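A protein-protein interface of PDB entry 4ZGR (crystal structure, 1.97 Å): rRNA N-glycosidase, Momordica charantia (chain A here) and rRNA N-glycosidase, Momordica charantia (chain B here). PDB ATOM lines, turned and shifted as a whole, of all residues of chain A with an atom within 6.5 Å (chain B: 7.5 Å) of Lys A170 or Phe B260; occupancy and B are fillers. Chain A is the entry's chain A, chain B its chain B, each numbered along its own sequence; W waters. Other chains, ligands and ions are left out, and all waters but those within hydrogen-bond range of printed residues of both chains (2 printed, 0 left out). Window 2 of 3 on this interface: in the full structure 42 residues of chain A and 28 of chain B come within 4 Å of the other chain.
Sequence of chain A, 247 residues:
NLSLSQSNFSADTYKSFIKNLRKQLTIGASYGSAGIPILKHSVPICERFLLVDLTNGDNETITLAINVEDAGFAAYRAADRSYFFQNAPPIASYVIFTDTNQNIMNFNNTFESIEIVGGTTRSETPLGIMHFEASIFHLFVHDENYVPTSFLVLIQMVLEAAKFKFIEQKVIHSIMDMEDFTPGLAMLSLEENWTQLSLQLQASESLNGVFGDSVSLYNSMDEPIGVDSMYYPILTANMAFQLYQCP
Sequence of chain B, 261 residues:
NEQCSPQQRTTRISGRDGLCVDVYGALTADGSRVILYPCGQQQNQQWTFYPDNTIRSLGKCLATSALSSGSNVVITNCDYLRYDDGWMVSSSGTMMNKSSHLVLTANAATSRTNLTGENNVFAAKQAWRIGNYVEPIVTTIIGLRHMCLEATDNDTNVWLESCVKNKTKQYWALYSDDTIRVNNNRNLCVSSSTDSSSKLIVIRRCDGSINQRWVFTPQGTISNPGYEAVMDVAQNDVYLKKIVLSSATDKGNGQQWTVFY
Printed residues of chain B within 4 Å of Phe A166: Phe B260 and Tyr B261. Of chain B, only Phe B260 (3.5 Å) comes within 4 Å of Lys A170. Printed residues of chain B within 4 Å of Ser A220: Tyr B261 (2.9 Å). Of the printed residues of chain A, Ile B142 touches Gln A169 (3.4 Å) and His A173 (3.9 Å). Of the printed residues of chain A, Phe B260 touches Phe A166, Gln A169, Lys A170 and His A173. Of the printed residues of chain A, Tyr B261 touches Phe A166 (3.5 Å) and Ser A220 (2.9 Å). The nearest residue of chain B that does not touch Lys A170 is Ile B142 (7.3 Å). The nearest printed residue of chain B that does not touch Phe A166 is Val B259 (4.8 Å).
The backbone NH (N) of Ser A220 sits at hydrogen-bond distance from the backbone carbonyl oxygen (O) of Tyr B261, 2.9 Å away.
O of Gln A169 lies within hydrogen-bond range of ND1 of His A173. OG1 of Thr B139 sits at hydrogen-bond distance from O of Phe B260, at 2.9 Å. N of Thr B140 lies within hydrogen-bond range of O of Phe B260, 2.9 Å away. The backbone carbonyl oxygen (O) of Ile B142 sits at hydrogen-bond distance from the backbone NH (N) of Thr B258 (2.7 Å).
Water W1 lies within hydrogen-bond range of O of Trp B257 (2.8 Å) and NZ of Lys A165 (2.9 Å). Water W2 lies within hydrogen-bond range of the side-chain hydroxyl (OG1) of Thr B140 (2.8 Å), a ring nitrogen (NE2) of His A173 (3.4 Å) and the side-chain sulfur (SG) of Cys B148 (3.7 Å).
Phe A166 touches Phe B260 (CE1 to CE1, 3.6 Å). CE1 of Tyr B261 touches CD1 of Phe A166, 3.5 Å away. NE2 of Gln A169 touches CD1 of Ile B142, at 3.4 Å. Phe B260 touches Gln A169 (CD1 to CG, 3.6 Å). CZ of Phe B260 touches CD of Lys A170, 3.5 Å away. His A173 touches Ile B142. Phe B260 touches His A173 (CE2 to CE1, 3.7 Å).
Printed residues of chain A that touch a printed residue of chain B: Phe A166, Gln A169, Lys A170, His A173 and Ser A220. Hydrophobic or aromatic side chains of chain A that line the printed part of chain B: Phe A166 and His A173. Of the 16 printed residues of chain B, 3 touch a printed residue of chain A. Among the printed residues, no Asp or Glu carboxylate lies within 4 Å of a Lys or Arg side-chain nitrogen of the other chain.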
ATOM      1  N   LYS A 165      -8.600   5.552  36.940  1.00  0.00           N
ATOM      2  CA  LYS A 165      -7.556   6.213  36.147  1.00  0.00           C
ATOM      3  C   LYS A 165      -8.131   7.273  35.195  1.00  0.00           C
ATOM      4  O   LYS A 165      -7.502   8.290  34.970  1.00  0.00           O
ATOM      5  CB  LYS A 165      -6.720   5.175  35.383  1.00  0.00           C
ATOM      6  CG  LYS A 165      -5.853   4.350  36.306  1.00  0.00           C
ATOM      7  CD  LYS A 165      -5.012   3.344  35.532  1.00  0.00           C
ATOM      8  CE  LYS A 165      -3.920   2.778  36.436  1.00  0.00           C
ATOM      9  NZ  LYS A 165      -3.180   1.642  35.815  1.00  0.00           N
ATOM     10  N   PHE A 166      -9.354   7.055  34.693  1.00  0.00           N
ATOM     11  CA  PHE A 166      -9.999   8.056  33.854  1.00  0.00           C
ATOM     12  C   PHE A 166     -10.126   9.388  34.587  1.00  0.00           C
ATOM     13  O   PHE A 166      -9.859  10.437  34.023  1.00  0.00           O
ATOM     14  CB  PHE A 166     -11.383   7.575  33.380  1.00  0.00           C
ATOM     15  CG  PHE A 166     -12.118   8.587  32.549  1.00  0.00           C
ATOM     16  CD1 PHE A 166     -11.937   8.638  31.159  1.00  0.00           C
ATOM     17  CD2 PHE A 166     -12.977   9.504  33.140  1.00  0.00           C
ATOM     18  CE1 PHE A 166     -12.617   9.574  30.387  1.00  0.00           C
ATOM     19  CE2 PHE A 166     -13.661  10.444  32.367  1.00  0.00           C
ATOM     20  CZ  PHE A 166     -13.475  10.474  30.997  1.00  0.00           C
ATOM     21  N   ILE A 167     -10.546   9.331  35.842  1.00  0.00           N
ATOM     22  CA  ILE A 167     -10.746  10.529  36.649  1.00  0.00           C
ATOM     23  C   ILE A 167      -9.409  11.174  37.014  1.00  0.00           C
ATOM     24  O   ILE A 167      -9.258  12.397  36.924  1.00  0.00           O
ATOM     25  CB  ILE A 167     -11.607  10.229  37.910  1.00  0.00           C
ATOM     26  CG1 ILE A 167     -13.019   9.816  37.453  1.00  0.00           C
ATOM     27  CG2 ILE A 167     -11.639  11.418  38.848  1.00  0.00           C
ATOM     28  CD1 ILE A 167     -13.988   9.395  38.544  1.00  0.00           C
ATOM     29  N   GLU A 168      -8.453  10.358  37.436  1.00  0.00           N
ATOM     30  CA  GLU A 168      -7.077  10.827  37.621  1.00  0.00           C
ATOM     31  C   GLU A 168      -6.601  11.644  36.393  1.00  0.00           C
ATOM     32  O   GLU A 168      -6.058  12.754  36.504  1.00  0.00           O
ATOM     33  CB  GLU A 168      -6.161   9.634  37.814  1.00  0.00           C
ATOM     34  CG  GLU A 168      -4.723  10.010  38.057  1.00  0.00           C
ATOM     35  CD  GLU A 168      -3.744   8.855  37.901  1.00  0.00           C
ATOM     36  OE1 GLU A 168      -4.129   7.671  37.773  1.00  0.00           O
ATOM     37  OE2 GLU A 168      -2.544   9.174  37.923  1.00  0.00           O
ATOM     38  N   GLN A 169      -6.808  11.065  35.226  1.00  0.00           N
ATOM     39  CA  GLN A 169      -6.397  11.690  33.992  1.00  0.00           C
ATOM     40  C   GLN A 169      -7.140  13.009  33.711  1.00  0.00           C
ATOM     41  O   GLN A 169      -6.541  13.968  33.182  1.00  0.00           O
ATOM     42  CB  GLN A 169      -6.553  10.723  32.834  1.00  0.00           C
ATOM     43  CG  GLN A 169      -5.840  11.195  31.578  1.00  0.00           C
ATOM     44  CD  GLN A 169      -4.354  11.423  31.789  1.00  0.00           C
ATOM     45  OE1 GLN A 169      -3.688  10.674  32.485  1.00  0.00           O
ATOM     46  NE2 GLN A 169      -3.846  12.480  31.202  1.00  0.00           N
ATOM     47  N   LYS A 170      -8.416  13.078  34.079  1.00  0.00           N
ATOM     48  CA  LYS A 170      -9.161  14.351  33.966  1.00  0.00           C
ATOM     49  C   LYS A 170      -8.500  15.442  34.783  1.00  0.00           C
ATOM     50  O   LYS A 170      -8.378  16.578  34.334  1.00  0.00           O
ATOM     51  CB  LYS A 170     -10.604  14.212  34.439  1.00  0.00           C
ATOM     52  CG  LYS A 170     -11.482  13.338  33.578  1.00  0.00           C
ATOM     53  CD  LYS A 170     -11.907  14.023  32.303  1.00  0.00           C
ATOM     54  CE  LYS A 170     -12.989  15.054  32.533  1.00  0.00           C
ATOM     55  NZ  LYS A 170     -13.258  15.718  31.232  1.00  0.00           N
ATOM     56  N   VAL A 171      -8.086  15.094  35.998  1.00  0.00           N
ATOM     57  CA  VAL A 171      -7.440  16.052  36.850  1.00  0.00           C
ATOM     58  C   VAL A 171      -6.077  16.452  36.240  1.00  0.00           C
ATOM     59  O   VAL A 171      -5.699  17.625  36.284  1.00  0.00           O
ATOM     60  CB  VAL A 171      -7.263  15.510  38.272  1.00  0.00           C
ATOM     61  CG1 VAL A 171      -6.475  16.486  39.118  1.00  0.00           C
ATOM     62  CG2 VAL A 171      -8.633  15.259  38.906  1.00  0.00           C
ATOM     63  N   ILE A 172      -5.358  15.473  35.690  1.00  0.00           N
ATOM     64  CA  ILE A 172      -4.044  15.723  35.099  1.00  0.00           C
ATOM     65  C   ILE A 172      -4.176  16.676  33.929  1.00  0.00           C
ATOM     66  O   ILE A 172      -3.366  17.592  33.793  1.00  0.00           O
ATOM     67  CB  ILE A 172      -3.351  14.414  34.675  1.00  0.00           C
ATOM     68  CG1 ILE A 172      -2.870  13.668  35.935  1.00  0.00           C
ATOM     69  CG2 ILE A 172      -2.208  14.668  33.664  1.00  0.00           C
ATOM     70  CD1 ILE A 172      -2.301  12.287  35.658  1.00  0.00           C
ATOM     71  N   HIS A 173      -5.177  16.454  33.085  1.00  0.00           N
ATOM     72  CA  HIS A 173      -5.466  17.387  32.010  1.00  0.00           C
ATOM     73  C   HIS A 173      -5.720  18.798  32.519  1.00  0.00           C
ATOM     74  O   HIS A 173      -5.212  19.773  31.950  1.00  0.00           O
ATOM     75  CB  HIS A 173      -6.643  16.908  31.179  1.00  0.00           C
ATOM     76  CG  HIS A 173      -6.312  15.792  30.243  1.00  0.00           C
ATOM     77  ND1 HIS A 173      -7.180  14.753  29.991  1.00  0.00           N
ATOM     78  CD2 HIS A 173      -5.222  15.562  29.478  1.00  0.00           C
ATOM     79  CE1 HIS A 173      -6.639  13.928  29.115  1.00  0.00           C
ATOM     80  NE2 HIS A 173      -5.452  14.399  28.782  1.00  0.00           N
ATOM     81  N   SER A 174      -6.501  18.907  33.583  1.00  0.00           N
ATOM     82  CA  SER A 174      -6.792  20.172  34.208  1.00  0.00           C
ATOM     83  C   SER A 174      -5.529  20.930  34.667  1.00  0.00           C
ATOM     84  O   SER A 174      -5.405  22.148  34.429  1.00  0.00           O
ATOM     85  CB  SER A 174      -7.701  19.944  35.404  1.00  0.00           C
ATOM     86  OG  SER A 174      -8.037  21.164  35.985  1.00  0.00           O
ATOM     87  N   ILE A 175      -4.622  20.208  35.322  1.00  0.00           N
ATOM     88  CA  ILE A 175      -3.366  20.774  35.798  1.00  0.00           C
ATOM     89  C   ILE A 175      -2.572  21.304  34.621  1.00  0.00           C
ATOM     90  O   ILE A 175      -2.137  22.452  34.615  1.00  0.00           O
ATOM     91  CB  ILE A 175      -2.488  19.725  36.517  1.00  0.00           C
ATOM     92  CG1 ILE A 175      -3.162  19.280  37.805  1.00  0.00           C
ATOM     93  CG2 ILE A 175      -1.100  20.309  36.828  1.00  0.00           C
ATOM     94  CD1 ILE A 175      -2.616  17.988  38.368  1.00  0.00           C
ATOM     95  N   GLU A 179      -6.812  24.638  33.465  1.00  0.00           N
ATOM     96  CA  GLU A 179      -8.164  24.762  32.981  1.00  0.00           C
ATOM     97  C   GLU A 179      -9.078  23.931  33.859  1.00  0.00           C
ATOM     98  O   GLU A 179      -8.928  22.713  33.949  1.00  0.00           O
ATOM     99  CB  GLU A 179      -8.209  24.271  31.546  1.00  0.00           C
ATOM    100  CG  GLU A 179      -9.453  24.638  30.795  1.00  0.00           C
ATOM    101  CD  GLU A 179      -9.271  24.398  29.309  1.00  0.00           C
ATOM    102  OE1 GLU A 179      -8.497  25.155  28.680  1.00  0.00           O
ATOM    103  OE2 GLU A 179      -9.876  23.446  28.782  1.00  0.00           O
ATOM    104  N   PHE A 181     -12.658  22.250  35.150  1.00  0.00           N
ATOM    105  CA  PHE A 181     -13.681  21.475  34.454  1.00  0.00           C
ATOM    106  C   PHE A 181     -14.756  21.066  35.454  1.00  0.00           C
ATOM    107  O   PHE A 181     -14.538  21.101  36.652  1.00  0.00           O
ATOM    108  CB  PHE A 181     -13.047  20.245  33.791  1.00  0.00           C
ATOM    109  CG  PHE A 181     -12.583  19.188  34.780  1.00  0.00           C
ATOM    110  CD1 PHE A 181     -11.405  19.367  35.517  1.00  0.00           C
ATOM    111  CD2 PHE A 181     -13.321  18.020  34.976  1.00  0.00           C
ATOM    112  CE1 PHE A 181     -10.968  18.410  36.424  1.00  0.00           C
ATOM    113  CE2 PHE A 181     -12.892  17.056  35.897  1.00  0.00           C
ATOM    114  CZ  PHE A 181     -11.720  17.252  36.622  1.00  0.00           C
ATOM    115  N   THR A 182     -15.926  20.699  34.952  1.00  0.00           N
ATOM    116  CA  THR A 182     -16.942  20.064  35.771  1.00  0.00           C
ATOM    117  C   THR A 182     -17.081  18.658  35.224  1.00  0.00           C
ATOM    118  O   THR A 182     -16.946  18.462  34.018  1.00  0.00           O
ATOM    119  CB  THR A 182     -18.282  20.798  35.706  1.00  0.00           C
ATOM    120  OG1 THR A 182     -18.636  20.997  34.341  1.00  0.00           O
ATOM    121  CG2 THR A 182     -18.163  22.149  36.395  1.00  0.00           C
ATOM    122  N   PRO A 183     -17.331  17.678  36.099  1.00  0.00           N
ATOM    123  CA  PRO A 183     -17.461  16.310  35.605  1.00  0.00           C
ATOM    124  C   PRO A 183     -18.657  16.178  34.686  1.00  0.00           C
ATOM    125  O   PRO A 183     -19.723  16.731  34.993  1.00  0.00           O
ATOM    126  CB  PRO A 183     -17.708  15.490  36.879  1.00  0.00           C
ATOM    127  CG  PRO A 183     -18.272  16.461  37.849  1.00  0.00           C
ATOM    128  CD  PRO A 183     -17.574  17.766  37.552  1.00  0.00           C
ATOM    129  N   GLY A 184     -18.465  15.459  33.589  1.00  0.00           N
ATOM    130  CA  GLY A 184     -19.528  15.143  32.663  1.00  0.00           C
ATOM    131  C   GLY A 184     -20.017  13.751  32.948  1.00  0.00           C
ATOM    132  O   GLY A 184     -19.660  13.154  33.980  1.00  0.00           O
ATOM    133  N   MET A 187     -17.358  10.818  33.787  1.00  0.00           N
ATOM    134  CA  MET A 187     -16.864  10.818  35.142  1.00  0.00           C
ATOM    135  C   MET A 187     -17.961  10.437  36.161  1.00  0.00           C
ATOM    136  O   MET A 187     -17.738   9.594  37.032  1.00  0.00           O
ATOM    137  CB  MET A 187     -16.221  12.168  35.434  1.00  0.00           C
ATOM    138  CG  MET A 187     -15.720  12.334  36.845  1.00  0.00           C
ATOM    139  SD  MET A 187     -14.457  13.612  36.905  1.00  0.00           S
ATOM    140  CE  MET A 187     -14.339  13.849  38.670  1.00  0.00           C
ATOM    141  N   SER A 220     -16.566  10.157  26.579  1.00  0.00           N
ATOM    142  CA  SER A 220     -16.439  11.604  26.530  1.00  0.00           C
ATOM    143  C   SER A 220     -17.328  12.289  25.462  1.00  0.00           C
ATOM    144  O   SER A 220     -17.494  13.499  25.507  1.00  0.00           O
ATOM    145  CB  SER A 220     -14.967  11.996  26.333  1.00  0.00           C
ATOM    146  OG  SER A 220     -14.286  11.894  27.571  1.00  0.00           O
ATOM    147  N   VAL B 138     -13.440   4.214  20.944  1.00  0.00           N
ATOM    148  CA  VAL B 138     -12.555   5.253  20.463  1.00  0.00           C
ATOM    149  C   VAL B 138     -11.867   5.939  21.629  1.00  0.00           C
ATOM    150  O   VAL B 138     -12.524   6.341  22.564  1.00  0.00           O
ATOM    151  CB  VAL B 138     -13.304   6.278  19.614  1.00  0.00           C
ATOM    152  CG1 VAL B 138     -12.381   7.408  19.153  1.00  0.00           C
ATOM    153  CG2 VAL B 138     -13.927   5.568  18.427  1.00  0.00           C
ATOM    154  N   THR B 139     -10.540   6.065  21.577  1.00  0.00           N
ATOM    155  CA  THR B 139      -9.796   6.545  22.731  1.00  0.00           C
ATOM    156  C   THR B 139      -8.482   7.240  22.379  1.00  0.00           C
ATOM    157  O   THR B 139      -7.981   7.137  21.248  1.00  0.00           O
ATOM    158  CB  THR B 139      -9.506   5.362  23.697  1.00  0.00           C
ATOM    159  OG1 THR B 139      -9.108   5.894  24.972  1.00  0.00           O
ATOM    160  CG2 THR B 139      -8.418   4.445  23.137  1.00  0.00           C
ATOM    161  N   THR B 140      -7.944   7.970  23.347  1.00  0.00           N
ATOM    162  CA  THR B 140      -6.530   8.344  23.330  1.00  0.00           C
ATOM    163  C   THR B 140      -5.811   7.389  24.277  1.00  0.00           C
ATOM    164  O   THR B 140      -6.426   6.763  25.146  1.00  0.00           O
ATOM    165  CB  THR B 140      -6.284   9.809  23.713  1.00  0.00           C
ATOM    166  OG1 THR B 140      -6.720  10.049  25.046  1.00  0.00           O
ATOM    167  CG2 THR B 140      -7.038  10.761  22.763  1.00  0.00           C
ATOM    168  N   ILE B 141      -4.506   7.266  24.069  1.00  0.00           N
ATOM    169  CA  ILE B 141      -3.668   6.349  24.827  1.00  0.00           C
ATOM    170  C   ILE B 141      -2.526   7.191  25.342  1.00  0.00           C
ATOM    171  O   ILE B 141      -1.705   7.666  24.561  1.00  0.00           O
ATOM    172  CB  ILE B 141      -3.148   5.202  23.971  1.00  0.00           C
ATOM    173  CG1 ILE B 141      -4.317   4.317  23.517  1.00  0.00           C
ATOM    174  CG2 ILE B 141      -2.148   4.377  24.774  1.00  0.00           C
ATOM    175  CD1 ILE B 141      -3.948   3.237  22.538  1.00  0.00           C
ATOM    176  N   ILE B 142      -2.494   7.377  26.647  1.00  0.00           N
ATOM    177  CA  ILE B 142      -1.601   8.314  27.286  1.00  0.00           C
ATOM    178  C   ILE B 142      -0.480   7.559  27.951  1.00  0.00           C
ATOM    179  O   ILE B 142      -0.715   6.544  28.584  1.00  0.00           O
ATOM    180  CB  ILE B 142      -2.354   9.155  28.317  1.00  0.00           C
ATOM    181  CG1 ILE B 142      -3.529   9.802  27.581  1.00  0.00           C
ATOM    182  CG2 ILE B 142      -1.433  10.213  28.933  1.00  0.00           C
ATOM    183  CD1 ILE B 142      -4.437  10.635  28.431  1.00  0.00           C
ATOM    184  N   CYS B 148       0.591  11.611  24.392  1.00  0.00           N
ATOM    185  CA  CYS B 148      -0.391  10.771  23.685  1.00  0.00           C
ATOM    186  C   CYS B 148       0.283   9.994  22.557  1.00  0.00           C
ATOM    187  O   CYS B 148       1.106  10.558  21.842  1.00  0.00           O
ATOM    188  CB  CYS B 148      -1.516  11.675  23.078  1.00  0.00           C
ATOM    189  SG  CYS B 148      -2.818  12.166  24.257  1.00  0.00           S
ATOM    190  N   LYS B 165      -6.399  17.949  22.054  1.00  0.00           N
ATOM    191  CA  LYS B 165      -7.789  17.515  21.959  1.00  0.00           C
ATOM    192  C   LYS B 165      -8.219  17.488  20.501  1.00  0.00           C
ATOM    193  O   LYS B 165      -7.929  18.415  19.753  1.00  0.00           O
ATOM    194  CB  LYS B 165      -8.675  18.472  22.750  1.00  0.00           C
ATOM    195  CG  LYS B 165     -10.121  18.036  22.915  1.00  0.00           C
ATOM    196  CD  LYS B 165     -10.829  18.897  23.966  1.00  0.00           C
ATOM    197  CE  LYS B 165     -12.344  18.878  23.797  1.00  0.00           C
ATOM    198  NZ  LYS B 165     -12.912  17.505  23.610  1.00  0.00           N
ATOM    199  N   GLN B 170      -4.232  11.200  16.995  1.00  0.00           N
ATOM    200  CA  GLN B 170      -4.071  10.750  18.383  1.00  0.00           C
ATOM    201  C   GLN B 170      -5.211   9.859  18.885  1.00  0.00           C
ATOM    202  O   GLN B 170      -5.204   9.466  20.044  1.00  0.00           O
ATOM    203  CB  GLN B 170      -3.887  11.951  19.293  1.00  0.00           C
ATOM    204  CG  GLN B 170      -2.586  12.658  19.026  1.00  0.00           C
ATOM    205  CD  GLN B 170      -2.257  13.774  19.984  1.00  0.00           C
ATOM    206  OE1 GLN B 170      -3.059  14.186  20.816  1.00  0.00           O
ATOM    207  NE2 GLN B 170      -1.038  14.280  19.868  1.00  0.00           N
ATOM    208  N   TYR B 171      -6.189   9.555  18.027  1.00  0.00           N
ATOM    209  CA  TYR B 171      -7.338   8.715  18.390  1.00  0.00           C
ATOM    210  C   TYR B 171      -7.160   7.327  17.856  1.00  0.00           C
ATOM    211  O   TYR B 171      -6.685   7.138  16.720  1.00  0.00           O
ATOM    212  CB  TYR B 171      -8.682   9.351  17.932  1.00  0.00           C
ATOM    213  CG  TYR B 171      -8.950  10.561  18.776  1.00  0.00           C
ATOM    214  CD1 TYR B 171      -8.289  11.744  18.515  1.00  0.00           C
ATOM    215  CD2 TYR B 171      -9.762  10.500  19.909  1.00  0.00           C
ATOM    216  CE1 TYR B 171      -8.438  12.852  19.319  1.00  0.00           C
ATOM    217  CE2 TYR B 171      -9.937  11.619  20.720  1.00  0.00           C
ATOM    218  CZ  TYR B 171      -9.265  12.790  20.416  1.00  0.00           C
ATOM    219  OH  TYR B 171      -9.392  13.938  21.182  1.00  0.00           O
ATOM    220  N   TRP B 172      -7.541   6.358  18.684  1.00  0.00           N
ATOM    221  CA  TRP B 172      -7.392   4.947  18.398  1.00  0.00           C
ATOM    222  C   TRP B 172      -8.718   4.235  18.614  1.00  0.00           C
ATOM    223  O   TRP B 172      -9.494   4.616  19.502  1.00  0.00           O
ATOM    224  CB  TRP B 172      -6.304   4.347  19.296  1.00  0.00           C
ATOM    225  CG  TRP B 172      -5.005   5.054  19.141  1.00  0.00           C
ATOM    226  CD1 TRP B 172      -4.566   6.118  19.867  1.00  0.00           C
ATOM    227  CD2 TRP B 172      -4.007   4.805  18.149  1.00  0.00           C
ATOM    228  NE1 TRP B 172      -3.341   6.530  19.414  1.00  0.00           N
ATOM    229  CE2 TRP B 172      -2.971   5.746  18.356  1.00  0.00           C
ATOM    230  CE3 TRP B 172      -3.889   3.888  17.104  1.00  0.00           C
ATOM    231  CZ2 TRP B 172      -1.810   5.788  17.554  1.00  0.00           C
ATOM    232  CZ3 TRP B 172      -2.724   3.923  16.313  1.00  0.00           C
ATOM    233  CH2 TRP B 172      -1.709   4.872  16.548  1.00  0.00           C
ATOM    234  N   LEU B 174     -10.258   0.794  19.659  1.00  0.00           N
ATOM    235  CA  LEU B 174      -9.995  -0.479  20.306  1.00  0.00           C
ATOM    236  C   LEU B 174     -11.055  -1.476  19.881  1.00  0.00           C
ATOM    237  O   LEU B 174     -12.214  -1.303  20.234  1.00  0.00           O
ATOM    238  CB  LEU B 174      -9.995  -0.290  21.843  1.00  0.00           C
ATOM    239  CG  LEU B 174      -9.070   0.780  22.430  1.00  0.00           C
ATOM    240  CD1 LEU B 174      -8.994   0.638  23.942  1.00  0.00           C
ATOM    241  CD2 LEU B 174      -7.667   0.663  21.825  1.00  0.00           C
ATOM    242  N   TRP B 257       0.649   3.092  30.851  1.00  0.00           N
ATOM    243  CA  TRP B 257      -0.235   3.716  29.874  1.00  0.00           C
ATOM    244  C   TRP B 257      -1.619   3.880  30.493  1.00  0.00           C
ATOM    245  O   TRP B 257      -1.980   3.145  31.405  1.00  0.00           O
ATOM    246  CB  TRP B 257      -0.331   2.849  28.623  1.00  0.00           C
ATOM    247  CG  TRP B 257       0.994   2.546  28.003  1.00  0.00           C
ATOM    248  CD1 TRP B 257       1.811   1.510  28.312  1.00  0.00           C
ATOM    249  CD2 TRP B 257       1.673   3.309  27.011  1.00  0.00           C
ATOM    250  NE1 TRP B 257       2.959   1.560  27.554  1.00  0.00           N
ATOM    251  CE2 TRP B 257       2.907   2.662  26.752  1.00  0.00           C
ATOM    252  CE3 TRP B 257       1.358   4.457  26.298  1.00  0.00           C
ATOM    253  CZ2 TRP B 257       3.815   3.129  25.797  1.00  0.00           C
ATOM    254  CZ3 TRP B 257       2.270   4.933  25.363  1.00  0.00           C
ATOM    255  CH2 TRP B 257       3.487   4.267  25.120  1.00  0.00           C
ATOM    256  N   THR B 258      -2.368   4.857  29.980  1.00  0.00           N
ATOM    257  CA  THR B 258      -3.759   5.130  30.403  1.00  0.00           C
ATOM    258  C   THR B 258      -4.661   5.219  29.164  1.00  0.00           C
ATOM    259  O   THR B 258      -4.308   5.857  28.182  1.00  0.00           O
ATOM    260  CB  THR B 258      -3.860   6.489  31.148  1.00  0.00           C
ATOM    261  OG1 THR B 258      -3.023   6.479  32.301  1.00  0.00           O
ATOM    262  CG2 THR B 258      -5.291   6.789  31.591  1.00  0.00           C
ATOM    263  N   VAL B 259      -5.835   4.612  29.241  1.00  0.00           N
ATOM    264  CA  VAL B 259      -6.840   4.739  28.213  1.00  0.00           C
ATOM    265  C   VAL B 259      -7.725   5.928  28.566  1.00  0.00           C
ATOM    266  O   VAL B 259      -8.362   5.912  29.617  1.00  0.00           O
ATOM    267  CB  VAL B 259      -7.657   3.456  28.139  1.00  0.00           C
ATOM    268  CG1 VAL B 259      -8.826   3.611  27.179  1.00  0.00           C
ATOM    269  CG2 VAL B 259      -6.769   2.327  27.668  1.00  0.00           C
ATOM    270  N   PHE B 260      -7.740   6.958  27.728  1.00  0.00           N
ATOM    271  CA  PHE B 260      -8.587   8.121  27.977  1.00  0.00           C
ATOM    272  C   PHE B 260      -9.659   8.249  26.887  1.00  0.00           C
ATOM    273  O   PHE B 260      -9.381   8.644  25.769  1.00  0.00           O
ATOM    274  CB  PHE B 260      -7.795   9.409  28.129  1.00  0.00           C
ATOM    275  CG  PHE B 260      -8.626  10.553  28.615  1.00  0.00           C
ATOM    276  CD1 PHE B 260      -8.962  10.648  29.947  1.00  0.00           C
ATOM    277  CD2 PHE B 260      -9.140  11.492  27.725  1.00  0.00           C
ATOM    278  CE1 PHE B 260      -9.755  11.685  30.413  1.00  0.00           C
ATOM    279  CE2 PHE B 260      -9.939  12.533  28.179  1.00  0.00           C
ATOM    280  CZ  PHE B 260     -10.259  12.626  29.527  1.00  0.00           C
ATOM    281  N   TYR B 261     -10.881   7.909  27.253  1.00  0.00           N
ATOM    282  CA  TYR B 261     -11.986   7.731  26.309  1.00  0.00           C
ATOM    283  C   TYR B 261     -13.012   8.862  26.487  1.00  0.00           C
ATOM    284  O   TYR B 261     -14.116   8.739  25.921  1.00  0.00           O
ATOM    285  CB  TYR B 261     -12.585   6.320  26.476  1.00  0.00           C
ATOM    286  CG  TYR B 261     -13.114   6.042  27.888  1.00  0.00           C
ATOM    287  CD1 TYR B 261     -12.278   5.562  28.906  1.00  0.00           C
ATOM    288  CD2 TYR B 261     -14.452   6.295  28.206  1.00  0.00           C
ATOM    289  CE1 TYR B 261     -12.748   5.346  30.196  1.00  0.00           C
ATOM    290  CE2 TYR B 261     -14.940   6.073  29.489  1.00  0.00           C
ATOM    291  CZ  TYR B 261     -14.090   5.611  30.487  1.00  0.00           C
ATOM    292  OH  TYR B 261     -14.607   5.418  31.746  1.00  0.00           O
HETATM  293  O   HOH W   1      -1.249   3.039  34.101  1.00  0.00           O
HETATM  294  O   HOH W   2      -6.068  12.629  25.951  1.00  0.00           O
